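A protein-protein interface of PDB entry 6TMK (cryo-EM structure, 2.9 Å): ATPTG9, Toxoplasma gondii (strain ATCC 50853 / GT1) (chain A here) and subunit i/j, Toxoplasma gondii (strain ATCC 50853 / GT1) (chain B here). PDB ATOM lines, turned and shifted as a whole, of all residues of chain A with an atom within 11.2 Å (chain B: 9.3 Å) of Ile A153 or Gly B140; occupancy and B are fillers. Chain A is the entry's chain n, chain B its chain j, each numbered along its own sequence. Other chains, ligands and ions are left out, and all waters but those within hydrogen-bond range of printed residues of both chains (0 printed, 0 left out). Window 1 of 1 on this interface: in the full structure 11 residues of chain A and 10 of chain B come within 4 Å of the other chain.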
ATOM      1  N   PRO A 148      23.946   2.741 -28.803  1.00  0.00           N
ATOM      2  CA  PRO A 148      23.600   2.160 -27.502  1.00  0.00           C
ATOM      3  C   PRO A 148      22.109   1.883 -27.420  1.00  0.00           C
ATOM      4  O   PRO A 148      21.288   2.804 -27.379  1.00  0.00           O
ATOM      5  CB  PRO A 148      24.035   3.250 -26.515  1.00  0.00           C
ATOM      6  CG  PRO A 148      23.853   4.499 -27.275  1.00  0.00           C
ATOM      7  CD  PRO A 148      24.205   4.185 -28.696  1.00  0.00           C
ATOM      8  N   GLY A 149      21.757   0.605 -27.394  1.00  0.00           N
ATOM      9  CA  GLY A 149      20.375   0.205 -27.513  1.00  0.00           C
ATOM     10  C   GLY A 149      20.215  -1.079 -28.295  1.00  0.00           C
ATOM     11  O   GLY A 149      19.144  -1.690 -28.296  1.00  0.00           O
ATOM     12  N   TYR A 150      21.282  -1.496 -28.969  1.00  0.00           N
ATOM     13  CA  TYR A 150      21.273  -2.765 -29.677  1.00  0.00           C
ATOM     14  C   TYR A 150      21.358  -3.920 -28.691  1.00  0.00           C
ATOM     15  O   TYR A 150      22.183  -3.909 -27.772  1.00  0.00           O
ATOM     16  CB  TYR A 150      22.425  -2.828 -30.676  1.00  0.00           C
ATOM     17  CG  TYR A 150      22.259  -3.926 -31.693  1.00  0.00           C
ATOM     18  CD1 TYR A 150      21.452  -3.745 -32.800  1.00  0.00           C
ATOM     19  CD2 TYR A 150      22.902  -5.142 -31.546  1.00  0.00           C
ATOM     20  CE1 TYR A 150      21.285  -4.738 -33.729  1.00  0.00           C
ATOM     21  CE2 TYR A 150      22.742  -6.145 -32.472  1.00  0.00           C
ATOM     22  CZ  TYR A 150      21.934  -5.939 -33.564  1.00  0.00           C
ATOM     23  OH  TYR A 150      21.769  -6.938 -34.495  1.00  0.00           O
ATOM     24  N   GLY A 151      20.498  -4.915 -28.881  1.00  0.00           N
ATOM     25  CA  GLY A 151      20.454  -6.061 -28.006  1.00  0.00           C
ATOM     26  C   GLY A 151      19.677  -5.859 -26.727  1.00  0.00           C
ATOM     27  O   GLY A 151      19.532  -6.813 -25.956  1.00  0.00           O
ATOM     28  N   HIS A 152      19.170  -4.658 -26.477  1.00  0.00           N
ATOM     29  CA  HIS A 152      18.363  -4.423 -25.292  1.00  0.00           C
ATOM     30  C   HIS A 152      16.978  -5.028 -25.459  1.00  0.00           C
ATOM     31  O   HIS A 152      16.314  -4.823 -26.478  1.00  0.00           O
ATOM     32  CB  HIS A 152      18.251  -2.927 -25.023  1.00  0.00           C
ATOM     33  CG  HIS A 152      17.350  -2.586 -23.884  1.00  0.00           C
ATOM     34  ND1 HIS A 152      16.256  -1.763 -24.027  1.00  0.00           N
ATOM     35  CD2 HIS A 152      17.375  -2.956 -22.582  1.00  0.00           C
ATOM     36  CE1 HIS A 152      15.646  -1.639 -22.863  1.00  0.00           C
ATOM     37  NE2 HIS A 152      16.306  -2.353 -21.969  1.00  0.00           N
ATOM     38  N   ILE A 153      16.552  -5.780 -24.455  1.00  0.00           N
ATOM     39  CA  ILE A 153      15.272  -6.468 -24.455  1.00  0.00           C
ATOM     40  C   ILE A 153      14.445  -5.929 -23.295  1.00  0.00           C
ATOM     41  O   ILE A 153      14.638  -6.324 -22.147  1.00  0.00           O
ATOM     42  CB  ILE A 153      15.453  -7.992 -24.351  1.00  0.00           C
ATOM     43  CG1 ILE A 153      16.296  -8.501 -25.515  1.00  0.00           C
ATOM     44  CG2 ILE A 153      14.113  -8.686 -24.354  1.00  0.00           C
ATOM     45  CD1 ILE A 153      16.786  -9.896 -25.332  1.00  0.00           C
ATOM     46  N   PRO A 154      13.508  -5.017 -23.557  1.00  0.00           N
ATOM     47  CA  PRO A 154      12.739  -4.442 -22.447  1.00  0.00           C
ATOM     48  C   PRO A 154      11.759  -5.409 -21.816  1.00  0.00           C
ATOM     49  O   PRO A 154      11.504  -5.305 -20.612  1.00  0.00           O
ATOM     50  CB  PRO A 154      12.021  -3.265 -23.111  1.00  0.00           C
ATOM     51  CG  PRO A 154      11.868  -3.678 -24.506  1.00  0.00           C
ATOM     52  CD  PRO A 154      13.128  -4.402 -24.836  1.00  0.00           C
ATOM     53  N   TYR A 155      11.197  -6.343 -22.580  1.00  0.00           N
ATOM     54  CA  TYR A 155      10.314  -7.348 -22.015  1.00  0.00           C
ATOM     55  C   TYR A 155      10.596  -8.683 -22.677  1.00  0.00           C
ATOM     56  O   TYR A 155      10.704  -8.764 -23.903  1.00  0.00           O
ATOM     57  CB  TYR A 155       8.838  -6.989 -22.190  1.00  0.00           C
ATOM     58  CG  TYR A 155       7.940  -8.073 -21.667  1.00  0.00           C
ATOM     59  CD1 TYR A 155       7.762  -8.244 -20.311  1.00  0.00           C
ATOM     60  CD2 TYR A 155       7.308  -8.950 -22.524  1.00  0.00           C
ATOM     61  CE1 TYR A 155       6.972  -9.232 -19.828  1.00  0.00           C
ATOM     62  CE2 TYR A 155       6.517  -9.945 -22.046  1.00  0.00           C
ATOM     63  CZ  TYR A 155       6.352 -10.089 -20.697  1.00  0.00           C
ATOM     64  OH  TYR A 155       5.552 -11.091 -20.220  1.00  0.00           O
ATOM     65  N   LYS A 156      10.699  -9.723 -21.861  1.00  0.00           N
ATOM     66  CA  LYS A 156      10.856 -11.086 -22.337  1.00  0.00           C
ATOM     67  C   LYS A 156       9.784 -11.968 -21.720  1.00  0.00           C
ATOM     68  O   LYS A 156       9.516 -11.892 -20.519  1.00  0.00           O
ATOM     69  CB  LYS A 156      12.237 -11.640 -21.996  1.00  0.00           C
ATOM     70  CG  LYS A 156      12.622 -12.885 -22.762  1.00  0.00           C
ATOM     71  CD  LYS A 156      13.932 -13.467 -22.253  1.00  0.00           C
ATOM     72  CE  LYS A 156      15.134 -12.857 -22.946  1.00  0.00           C
ATOM     73  NZ  LYS A 156      15.218 -13.239 -24.377  1.00  0.00           N
ATOM     74  N   TRP A 157       9.176 -12.802 -22.555  1.00  0.00           N
ATOM     75  CA  TRP A 157       8.188 -13.760 -22.085  1.00  0.00           C
ATOM     76  C   TRP A 157       8.785 -14.630 -20.987  1.00  0.00           C
ATOM     77  O   TRP A 157       9.861 -15.209 -21.150  1.00  0.00           O
ATOM     78  CB  TRP A 157       7.725 -14.614 -23.258  1.00  0.00           C
ATOM     79  CG  TRP A 157       6.645 -15.580 -22.967  1.00  0.00           C
ATOM     80  CD1 TRP A 157       6.776 -16.806 -22.405  1.00  0.00           C
ATOM     81  CD2 TRP A 157       5.259 -15.422 -23.265  1.00  0.00           C
ATOM     82  NE1 TRP A 157       5.561 -17.419 -22.319  1.00  0.00           N
ATOM     83  CE2 TRP A 157       4.610 -16.589 -22.844  1.00  0.00           C
ATOM     84  CE3 TRP A 157       4.504 -14.406 -23.846  1.00  0.00           C
ATOM     85  CZ2 TRP A 157       3.245 -16.763 -22.979  1.00  0.00           C
ATOM     86  CZ3 TRP A 157       3.163 -14.585 -23.978  1.00  0.00           C
ATOM     87  CH2 TRP A 157       2.543 -15.751 -23.547  1.00  0.00           C
ATOM     88  N   GLU A 158       8.080 -14.719 -19.865  1.00  0.00           N
ATOM     89  CA  GLU A 158       8.617 -15.384 -18.688  1.00  0.00           C
ATOM     90  C   GLU A 158       8.594 -16.890 -18.897  1.00  0.00           C
ATOM     91  O   GLU A 158       7.535 -17.477 -19.139  1.00  0.00           O
ATOM     92  CB  GLU A 158       7.814 -14.983 -17.458  1.00  0.00           C
ATOM     93  CG  GLU A 158       7.672 -13.478 -17.319  1.00  0.00           C
ATOM     94  CD  GLU A 158       6.809 -13.069 -16.153  1.00  0.00           C
ATOM     95  OE1 GLU A 158       6.664 -13.873 -15.208  1.00  0.00           O
ATOM     96  OE2 GLU A 158       6.272 -11.940 -16.185  1.00  0.00           O
ATOM     97  N   ARG A 161      12.972 -21.405 -20.384  1.00  0.00           N
ATOM     98  CA  ARG A 161      13.838 -21.331 -21.542  1.00  0.00           C
ATOM     99  C   ARG A 161      14.437 -19.930 -21.640  1.00  0.00           C
ATOM    100  O   ARG A 161      13.745 -18.942 -21.385  1.00  0.00           O
ATOM    101  CB  ARG A 161      13.058 -21.658 -22.809  1.00  0.00           C
ATOM    102  CG  ARG A 161      13.908 -21.742 -24.038  1.00  0.00           C
ATOM    103  CD  ARG A 161      13.126 -22.299 -25.184  1.00  0.00           C
ATOM    104  NE  ARG A 161      13.805 -22.073 -26.452  1.00  0.00           N
ATOM    105  CZ  ARG A 161      13.219 -22.148 -27.637  1.00  0.00           C
ATOM    106  NH1 ARG A 161      11.937 -22.446 -27.731  1.00  0.00           N
ATOM    107  NH2 ARG A 161      13.924 -21.924 -28.728  1.00  0.00           N
ATOM    108  N   PRO A 162      15.709 -19.807 -22.012  1.00  0.00           N
ATOM    109  CA  PRO A 162      16.301 -18.471 -22.137  1.00  0.00           C
ATOM    110  C   PRO A 162      15.675 -17.637 -23.239  1.00  0.00           C
ATOM    111  O   PRO A 162      15.361 -16.460 -23.032  1.00  0.00           O
ATOM    112  CB  PRO A 162      17.775 -18.773 -22.433  1.00  0.00           C
ATOM    113  CG  PRO A 162      17.987 -20.135 -21.895  1.00  0.00           C
ATOM    114  CD  PRO A 162      16.723 -20.858 -22.171  1.00  0.00           C
ATOM    115  N   ASN A 163      15.500 -18.233 -24.419  1.00  0.00           N
ATOM    116  CA  ASN A 163      14.918 -17.560 -25.575  1.00  0.00           C
ATOM    117  C   ASN A 163      13.582 -18.205 -25.907  1.00  0.00           C
ATOM    118  O   ASN A 163      13.534 -19.202 -26.641  1.00  0.00           O
ATOM    119  CB  ASN A 163      15.866 -17.621 -26.772  1.00  0.00           C
ATOM    120  CG  ASN A 163      16.778 -16.422 -26.850  1.00  0.00           C
ATOM    121  OD1 ASN A 163      16.362 -15.340 -27.259  1.00  0.00           O
ATOM    122  ND2 ASN A 163      18.031 -16.602 -26.449  1.00  0.00           N
ATOM    123  N   PRO A 164      12.469 -17.685 -25.399  1.00  0.00           N
ATOM    124  CA  PRO A 164      11.171 -18.279 -25.727  1.00  0.00           C
ATOM    125  C   PRO A 164      10.837 -18.062 -27.192  1.00  0.00           C
ATOM    126  O   PRO A 164      11.071 -16.989 -27.750  1.00  0.00           O
ATOM    127  CB  PRO A 164      10.197 -17.537 -24.807  1.00  0.00           C
ATOM    128  CG  PRO A 164      11.047 -16.935 -23.759  1.00  0.00           C
ATOM    129  CD  PRO A 164      12.326 -16.600 -24.423  1.00  0.00           C
ATOM    130  N   GLY A 165      10.285 -19.095 -27.816  1.00  0.00           N
ATOM    131  CA  GLY A 165      10.130 -19.073 -29.252  1.00  0.00           C
ATOM    132  C   GLY A 165      11.446 -19.412 -29.915  1.00  0.00           C
ATOM    133  O   GLY A 165      11.859 -20.574 -29.943  1.00  0.00           O
ATOM    134  N   ALA A 166      12.118 -18.402 -30.449  1.00  0.00           N
ATOM    135  CA  ALA A 166      13.422 -18.595 -31.060  1.00  0.00           C
ATOM    136  C   ALA A 166      14.456 -18.944 -30.001  1.00  0.00           C
ATOM    137  O   ALA A 166      15.581 -18.444 -30.033  1.00  0.00           O
ATOM    138  CB  ALA A 166      13.845 -17.351 -31.810  1.00  0.00           C
ATOM    139  OXT ALA A 166      14.196 -19.733 -29.095  1.00  0.00           O
ATOM    140  N   SER B 134       4.390 -13.327 -34.639  1.00  0.00           N
ATOM    141  CA  SER B 134       5.642 -12.698 -35.030  1.00  0.00           C
ATOM    142  C   SER B 134       6.329 -12.087 -33.818  1.00  0.00           C
ATOM    143  O   SER B 134       7.530 -12.288 -33.599  1.00  0.00           O
ATOM    144  CB  SER B 134       5.377 -11.647 -36.103  1.00  0.00           C
ATOM    145  OG  SER B 134       4.639 -12.185 -37.174  1.00  0.00           O
ATOM    146  N   ALA B 135       5.572 -11.351 -33.006  1.00  0.00           N
ATOM    147  CA  ALA B 135       6.144 -10.745 -31.812  1.00  0.00           C
ATOM    148  C   ALA B 135       6.643 -11.802 -30.834  1.00  0.00           C
ATOM    149  O   ALA B 135       7.675 -11.617 -30.183  1.00  0.00           O
ATOM    150  CB  ALA B 135       5.106  -9.845 -31.153  1.00  0.00           C
ATOM    151  N   PHE B 136       5.928 -12.922 -30.726  1.00  0.00           N
ATOM    152  CA  PHE B 136       6.299 -13.971 -29.784  1.00  0.00           C
ATOM    153  C   PHE B 136       7.576 -14.678 -30.210  1.00  0.00           C
ATOM    154  O   PHE B 136       8.467 -14.916 -29.389  1.00  0.00           O
ATOM    155  CB  PHE B 136       5.155 -14.974 -29.640  1.00  0.00           C
ATOM    156  CG  PHE B 136       5.443 -16.079 -28.680  1.00  0.00           C
ATOM    157  CD1 PHE B 136       5.293 -15.894 -27.324  1.00  0.00           C
ATOM    158  CD2 PHE B 136       5.877 -17.304 -29.133  1.00  0.00           C
ATOM    159  CE1 PHE B 136       5.569 -16.902 -26.451  1.00  0.00           C
ATOM    160  CE2 PHE B 136       6.154 -18.307 -28.262  1.00  0.00           C
ATOM    161  CZ  PHE B 136       6.000 -18.108 -26.917  1.00  0.00           C
ATOM    162  N   HIS B 137       7.678 -15.039 -31.484  1.00  0.00           N
ATOM    163  CA  HIS B 137       8.845 -15.759 -31.966  1.00  0.00           C
ATOM    164  C   HIS B 137      10.001 -14.842 -32.329  1.00  0.00           C
ATOM    165  O   HIS B 137      11.061 -15.338 -32.720  1.00  0.00           O
ATOM    166  CB  HIS B 137       8.463 -16.641 -33.149  1.00  0.00           C
ATOM    167  CG  HIS B 137       7.590 -17.793 -32.771  1.00  0.00           C
ATOM    168  ND1 HIS B 137       8.063 -18.884 -32.079  1.00  0.00           N
ATOM    169  CD2 HIS B 137       6.272 -18.017 -32.970  1.00  0.00           C
ATOM    170  CE1 HIS B 137       7.075 -19.733 -31.873  1.00  0.00           C
ATOM    171  NE2 HIS B 137       5.978 -19.231 -32.405  1.00  0.00           N
ATOM    172  N   ASN B 138       9.829 -13.525 -32.204  1.00  0.00           N
ATOM    173  CA  ASN B 138      10.935 -12.573 -32.215  1.00  0.00           C
ATOM    174  C   ASN B 138      10.895 -11.824 -30.888  1.00  0.00           C
ATOM    175  O   ASN B 138      10.360 -10.709 -30.802  1.00  0.00           O
ATOM    176  CB  ASN B 138      10.839 -11.635 -33.408  1.00  0.00           C
ATOM    177  CG  ASN B 138      10.945 -12.371 -34.718  1.00  0.00           C
ATOM    178  OD1 ASN B 138      12.035 -12.628 -35.221  1.00  0.00           O
ATOM    179  ND2 ASN B 138       9.806 -12.743 -35.265  1.00  0.00           N
ATOM    180  N   PRO B 139      11.474 -12.401 -29.839  1.00  0.00           N
ATOM    181  CA  PRO B 139      11.222 -11.932 -28.471  1.00  0.00           C
ATOM    182  C   PRO B 139      11.447 -10.451 -28.205  1.00  0.00           C
ATOM    183  O   PRO B 139      10.526  -9.765 -27.754  1.00  0.00           O
ATOM    184  CB  PRO B 139      12.199 -12.784 -27.658  1.00  0.00           C
ATOM    185  CG  PRO B 139      12.234 -14.049 -28.386  1.00  0.00           C
ATOM    186  CD  PRO B 139      12.250 -13.649 -29.829  1.00  0.00           C
ATOM    187  N   GLY B 140      12.647  -9.945 -28.449  1.00  0.00           N
ATOM    188  CA  GLY B 140      12.955  -8.589 -28.042  1.00  0.00           C
ATOM    189  C   GLY B 140      12.994  -7.595 -29.178  1.00  0.00           C
ATOM    190  O   GLY B 140      13.669  -6.566 -29.083  1.00  0.00           O
ATOM    191  N   LYS B 141      12.271  -7.882 -30.247  1.00  0.00           N
ATOM    192  CA  LYS B 141      12.354  -7.115 -31.474  1.00  0.00           C
ATOM    193  C   LYS B 141      10.980  -6.578 -31.858  1.00  0.00           C
ATOM    194  O   LYS B 141       9.975  -6.824 -31.191  1.00  0.00           O
ATOM    195  CB  LYS B 141      12.948  -7.970 -32.590  1.00  0.00           C
ATOM    196  CG  LYS B 141      14.385  -8.376 -32.334  1.00  0.00           C
ATOM    197  CD  LYS B 141      14.652  -9.776 -32.805  1.00  0.00           C
ATOM    198  CE  LYS B 141      15.970 -10.296 -32.290  1.00  0.00           C
ATOM    199  NZ  LYS B 141      17.099  -9.432 -32.688  1.00  0.00           N
ATOM    200  N   ARG B 142      10.963  -5.829 -32.956  1.00  0.00           N
ATOM    201  CA  ARG B 142       9.776  -5.131 -33.443  1.00  0.00           C
ATOM    202  C   ARG B 142       9.585  -5.485 -34.909  1.00  0.00           C
ATOM    203  O   ARG B 142      10.279  -4.929 -35.778  1.00  0.00           O
ATOM    204  CB  ARG B 142       9.907  -3.629 -33.259  1.00  0.00           C
ATOM    205  CG  ARG B 142       9.876  -3.182 -31.827  1.00  0.00           C
ATOM    206  CD  ARG B 142      10.042  -1.697 -31.709  1.00  0.00           C
ATOM    207  NE  ARG B 142       8.926  -0.962 -32.283  1.00  0.00           N
ATOM    208  CZ  ARG B 142       7.770  -0.750 -31.671  1.00  0.00           C
ATOM    209  NH1 ARG B 142       6.823  -0.067 -32.278  1.00  0.00           N
ATOM    210  NH2 ARG B 142       7.557  -1.216 -30.458  1.00  0.00           N
ATOM    211  N   PRO B 143       8.678  -6.396 -35.228  1.00  0.00           N
ATOM    212  CA  PRO B 143       8.625  -6.924 -36.593  1.00  0.00           C
ATOM    213  C   PRO B 143       7.776  -6.126 -37.567  1.00  0.00           C
ATOM    214  O   PRO B 143       7.439  -6.638 -38.636  1.00  0.00           O
ATOM    215  CB  PRO B 143       8.051  -8.329 -36.381  1.00  0.00           C
ATOM    216  CG  PRO B 143       7.194  -8.187 -35.210  1.00  0.00           C
ATOM    217  CD  PRO B 143       7.818  -7.172 -34.318  1.00  0.00           C
ATOM    218  N   VAL B 183      15.004   3.338 -31.496  1.00  0.00           N
ATOM    219  CA  VAL B 183      15.015   2.316 -30.460  1.00  0.00           C
ATOM    220  C   VAL B 183      16.424   1.794 -30.237  1.00  0.00           C
ATOM    221  O   VAL B 183      16.809   1.476 -29.106  1.00  0.00           O
ATOM    222  CB  VAL B 183      14.038   1.186 -30.826  1.00  0.00           C
ATOM    223  CG1 VAL B 183      14.317  -0.029 -30.013  1.00  0.00           C
ATOM    224  CG2 VAL B 183      12.622   1.633 -30.609  1.00  0.00           C
ATOM    225  N   ASN B 184      17.216   1.700 -31.302  1.00  0.00           N
ATOM    226  CA  ASN B 184      18.596   1.261 -31.143  1.00  0.00           C
ATOM    227  C   ASN B 184      19.533   2.382 -30.713  1.00  0.00           C
ATOM    228  O   ASN B 184      20.604   2.102 -30.170  1.00  0.00           O
ATOM    229  CB  ASN B 184      19.088   0.610 -32.428  1.00  0.00           C
ATOM    230  CG  ASN B 184      18.620  -0.815 -32.559  1.00  0.00           C
ATOM    231  OD1 ASN B 184      19.283  -1.740 -32.106  1.00  0.00           O
ATOM    232  ND2 ASN B 184      17.460  -1.001 -33.162  1.00  0.00           N
ATOM    233  N   GLU B 187      18.489   4.095 -25.497  1.00  0.00           N
ATOM    234  CA  GLU B 187      18.117   2.929 -24.717  1.00  0.00           C
ATOM    235  C   GLU B 187      16.933   3.262 -23.822  1.00  0.00           C
ATOM    236  O   GLU B 187      16.980   4.217 -23.042  1.00  0.00           O
ATOM    237  CB  GLU B 187      19.298   2.473 -23.868  1.00  0.00           C
ATOM    238  CG  GLU B 187      19.298   1.006 -23.514  1.00  0.00           C
ATOM    239  CD  GLU B 187      20.525   0.603 -22.727  1.00  0.00           C
ATOM    240  OE1 GLU B 187      21.390   1.470 -22.489  1.00  0.00           O
ATOM    241  OE2 GLU B 187      20.623  -0.580 -22.338  1.00  0.00           O
ATOM    242  N   GLY B 188      15.874   2.467 -23.932  1.00  0.00           N
ATOM    243  CA  GLY B 188      14.719   2.633 -23.089  1.00  0.00           C
ATOM    244  C   GLY B 188      13.678   3.608 -23.581  1.00  0.00           C
ATOM    245  O   GLY B 188      12.756   3.928 -22.824  1.00  0.00           O
ATOM    246  N   ARG B 196       5.592   2.179 -28.105  1.00  0.00           N
ATOM    247  CA  ARG B 196       6.184   1.119 -27.311  1.00  0.00           C
ATOM    248  C   ARG B 196       5.909   1.413 -25.849  1.00  0.00           C
ATOM    249  O   ARG B 196       6.020   2.558 -25.414  1.00  0.00           O
ATOM    250  CB  ARG B 196       7.690   1.019 -27.573  1.00  0.00           C
ATOM    251  CG  ARG B 196       8.418   0.034 -26.710  1.00  0.00           C
ATOM    252  CD  ARG B 196       9.720  -0.415 -27.299  1.00  0.00           C
ATOM    253  NE  ARG B 196      10.854   0.372 -26.847  1.00  0.00           N
ATOM    254  CZ  ARG B 196      12.110  -0.048 -26.889  1.00  0.00           C
ATOM    255  NH1 ARG B 196      12.397  -1.245 -27.365  1.00  0.00           N
ATOM    256  NH2 ARG B 196      13.079   0.735 -26.460  1.00  0.00           N
ATOM    257  N   PHE B 198       6.577  -0.501 -21.922  1.00  0.00           N
ATOM    258  CA  PHE B 198       7.008  -1.558 -21.028  1.00  0.00           C
ATOM    259  C   PHE B 198       7.061  -1.025 -19.604  1.00  0.00           C
ATOM    260  O   PHE B 198       7.203   0.175 -19.368  1.00  0.00           O
ATOM    261  CB  PHE B 198       8.351  -2.175 -21.460  1.00  0.00           C
ATOM    262  CG  PHE B 198       9.456  -1.196 -21.628  1.00  0.00           C
ATOM    263  CD1 PHE B 198      10.293  -0.899 -20.581  1.00  0.00           C
ATOM    264  CD2 PHE B 198       9.684  -0.600 -22.844  1.00  0.00           C
ATOM    265  CE1 PHE B 198      11.310  -0.017 -20.737  1.00  0.00           C
ATOM    266  CE2 PHE B 198      10.702   0.285 -23.001  1.00  0.00           C
ATOM    267  CZ  PHE B 198      11.518   0.577 -21.952  1.00  0.00           C
ATOM    268  N   ARG B 200       8.959  -2.411 -16.643  1.00  0.00           N
ATOM    269  CA  ARG B 200      10.190  -2.431 -15.856  1.00  0.00           C
ATOM    270  C   ARG B 200      11.118  -1.359 -16.405  1.00  0.00           C
ATOM    271  O   ARG B 200      11.951  -1.603 -17.277  1.00  0.00           O
ATOM    272  CB  ARG B 200      10.833  -3.808 -15.888  1.00  0.00           C
ATOM    273  CG  ARG B 200       9.999  -4.872 -15.234  1.00  0.00           C
ATOM    274  CD  ARG B 200      10.069  -4.780 -13.738  1.00  0.00           C
ATOM    275  NE  ARG B 200       8.817  -5.201 -13.119  1.00  0.00           N
ATOM    276  CZ  ARG B 200       8.483  -4.947 -11.859  1.00  0.00           C
ATOM    277  NH1 ARG B 200       9.308  -4.268 -11.074  1.00  0.00           N
ATOM    278  NH2 ARG B 200       7.319  -5.371 -11.386  1.00  0.00           N
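Among the printed residues, pairs that only touch across the chains: Pro A148 with Glu B187, Tyr A150 with Asn B184, Ile A153 with Gly B140, Pro A154 with Arg B196, Pro A154 with Phe B198, Tyr A155 with Pro B139, Trp A157 with Phe B136, Pro A164 with Phe B136, Pro A164 with Pro B139, Gly A165 with His B137 and Ala A166 with His B137.
O of Asn B184 lies close to N of Gly A149 (3.4 Å).
O of Asn B184 lies close to O of Pro A148.
The guanidinium group (NH2) of Arg A161 lies within hydrogen-bond range of the backbone carbonyl oxygen (O) of Gly A165 (2.8 Å).
The guanidinium group of Arg A161 lies within salt-bridge range of the chain-end carboxylate of Ala A166 (3.6 Å).
Printed residues of chain B within 4 Å of Pro A148: Asn B184 (3.0 Å) and Glu B187 (3.6 Å).
No residue of chain B comes within 4 Å of His A152.
Printed residues of chain B within 4 Å of Ile A153: Gly B140.
Glu A158 touches none of the printed residues of chain B.
Ser B134 touches none of the printed residues of chain A.
Printed residues of chain A within 4 Å of His B137: Gly A165 and Ala A166.
Of the printed residues of chain A, Pro B139 touches Tyr A155 and Pro A164.
Gly B140 touches one residue of chain A.
Of the printed residues of chain A, Asn B184 touches Pro A148 (3.0 Å), Gly A149 (3.3 Å) and Tyr A150 (3.0 Å).
The nearest residue of chain B that does not touch Ile A153 is Pro B139 (5.0 Å).
The nearest residue of chain A that does not touch Gly B140 is His A152 (4.1 Å).
Hydrophobic or aromatic side chains of chain B within 4 Å of the printed part of chain A: Phe B136, His B137, Pro B139 and Phe B198.
Among the printed residues, 13 pairs touch across the chains.
Among the printed residues, no Asp or Glu carboxylate lies within 4 Å of a Lys or Arg side-chain nitrogen of the other chain.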
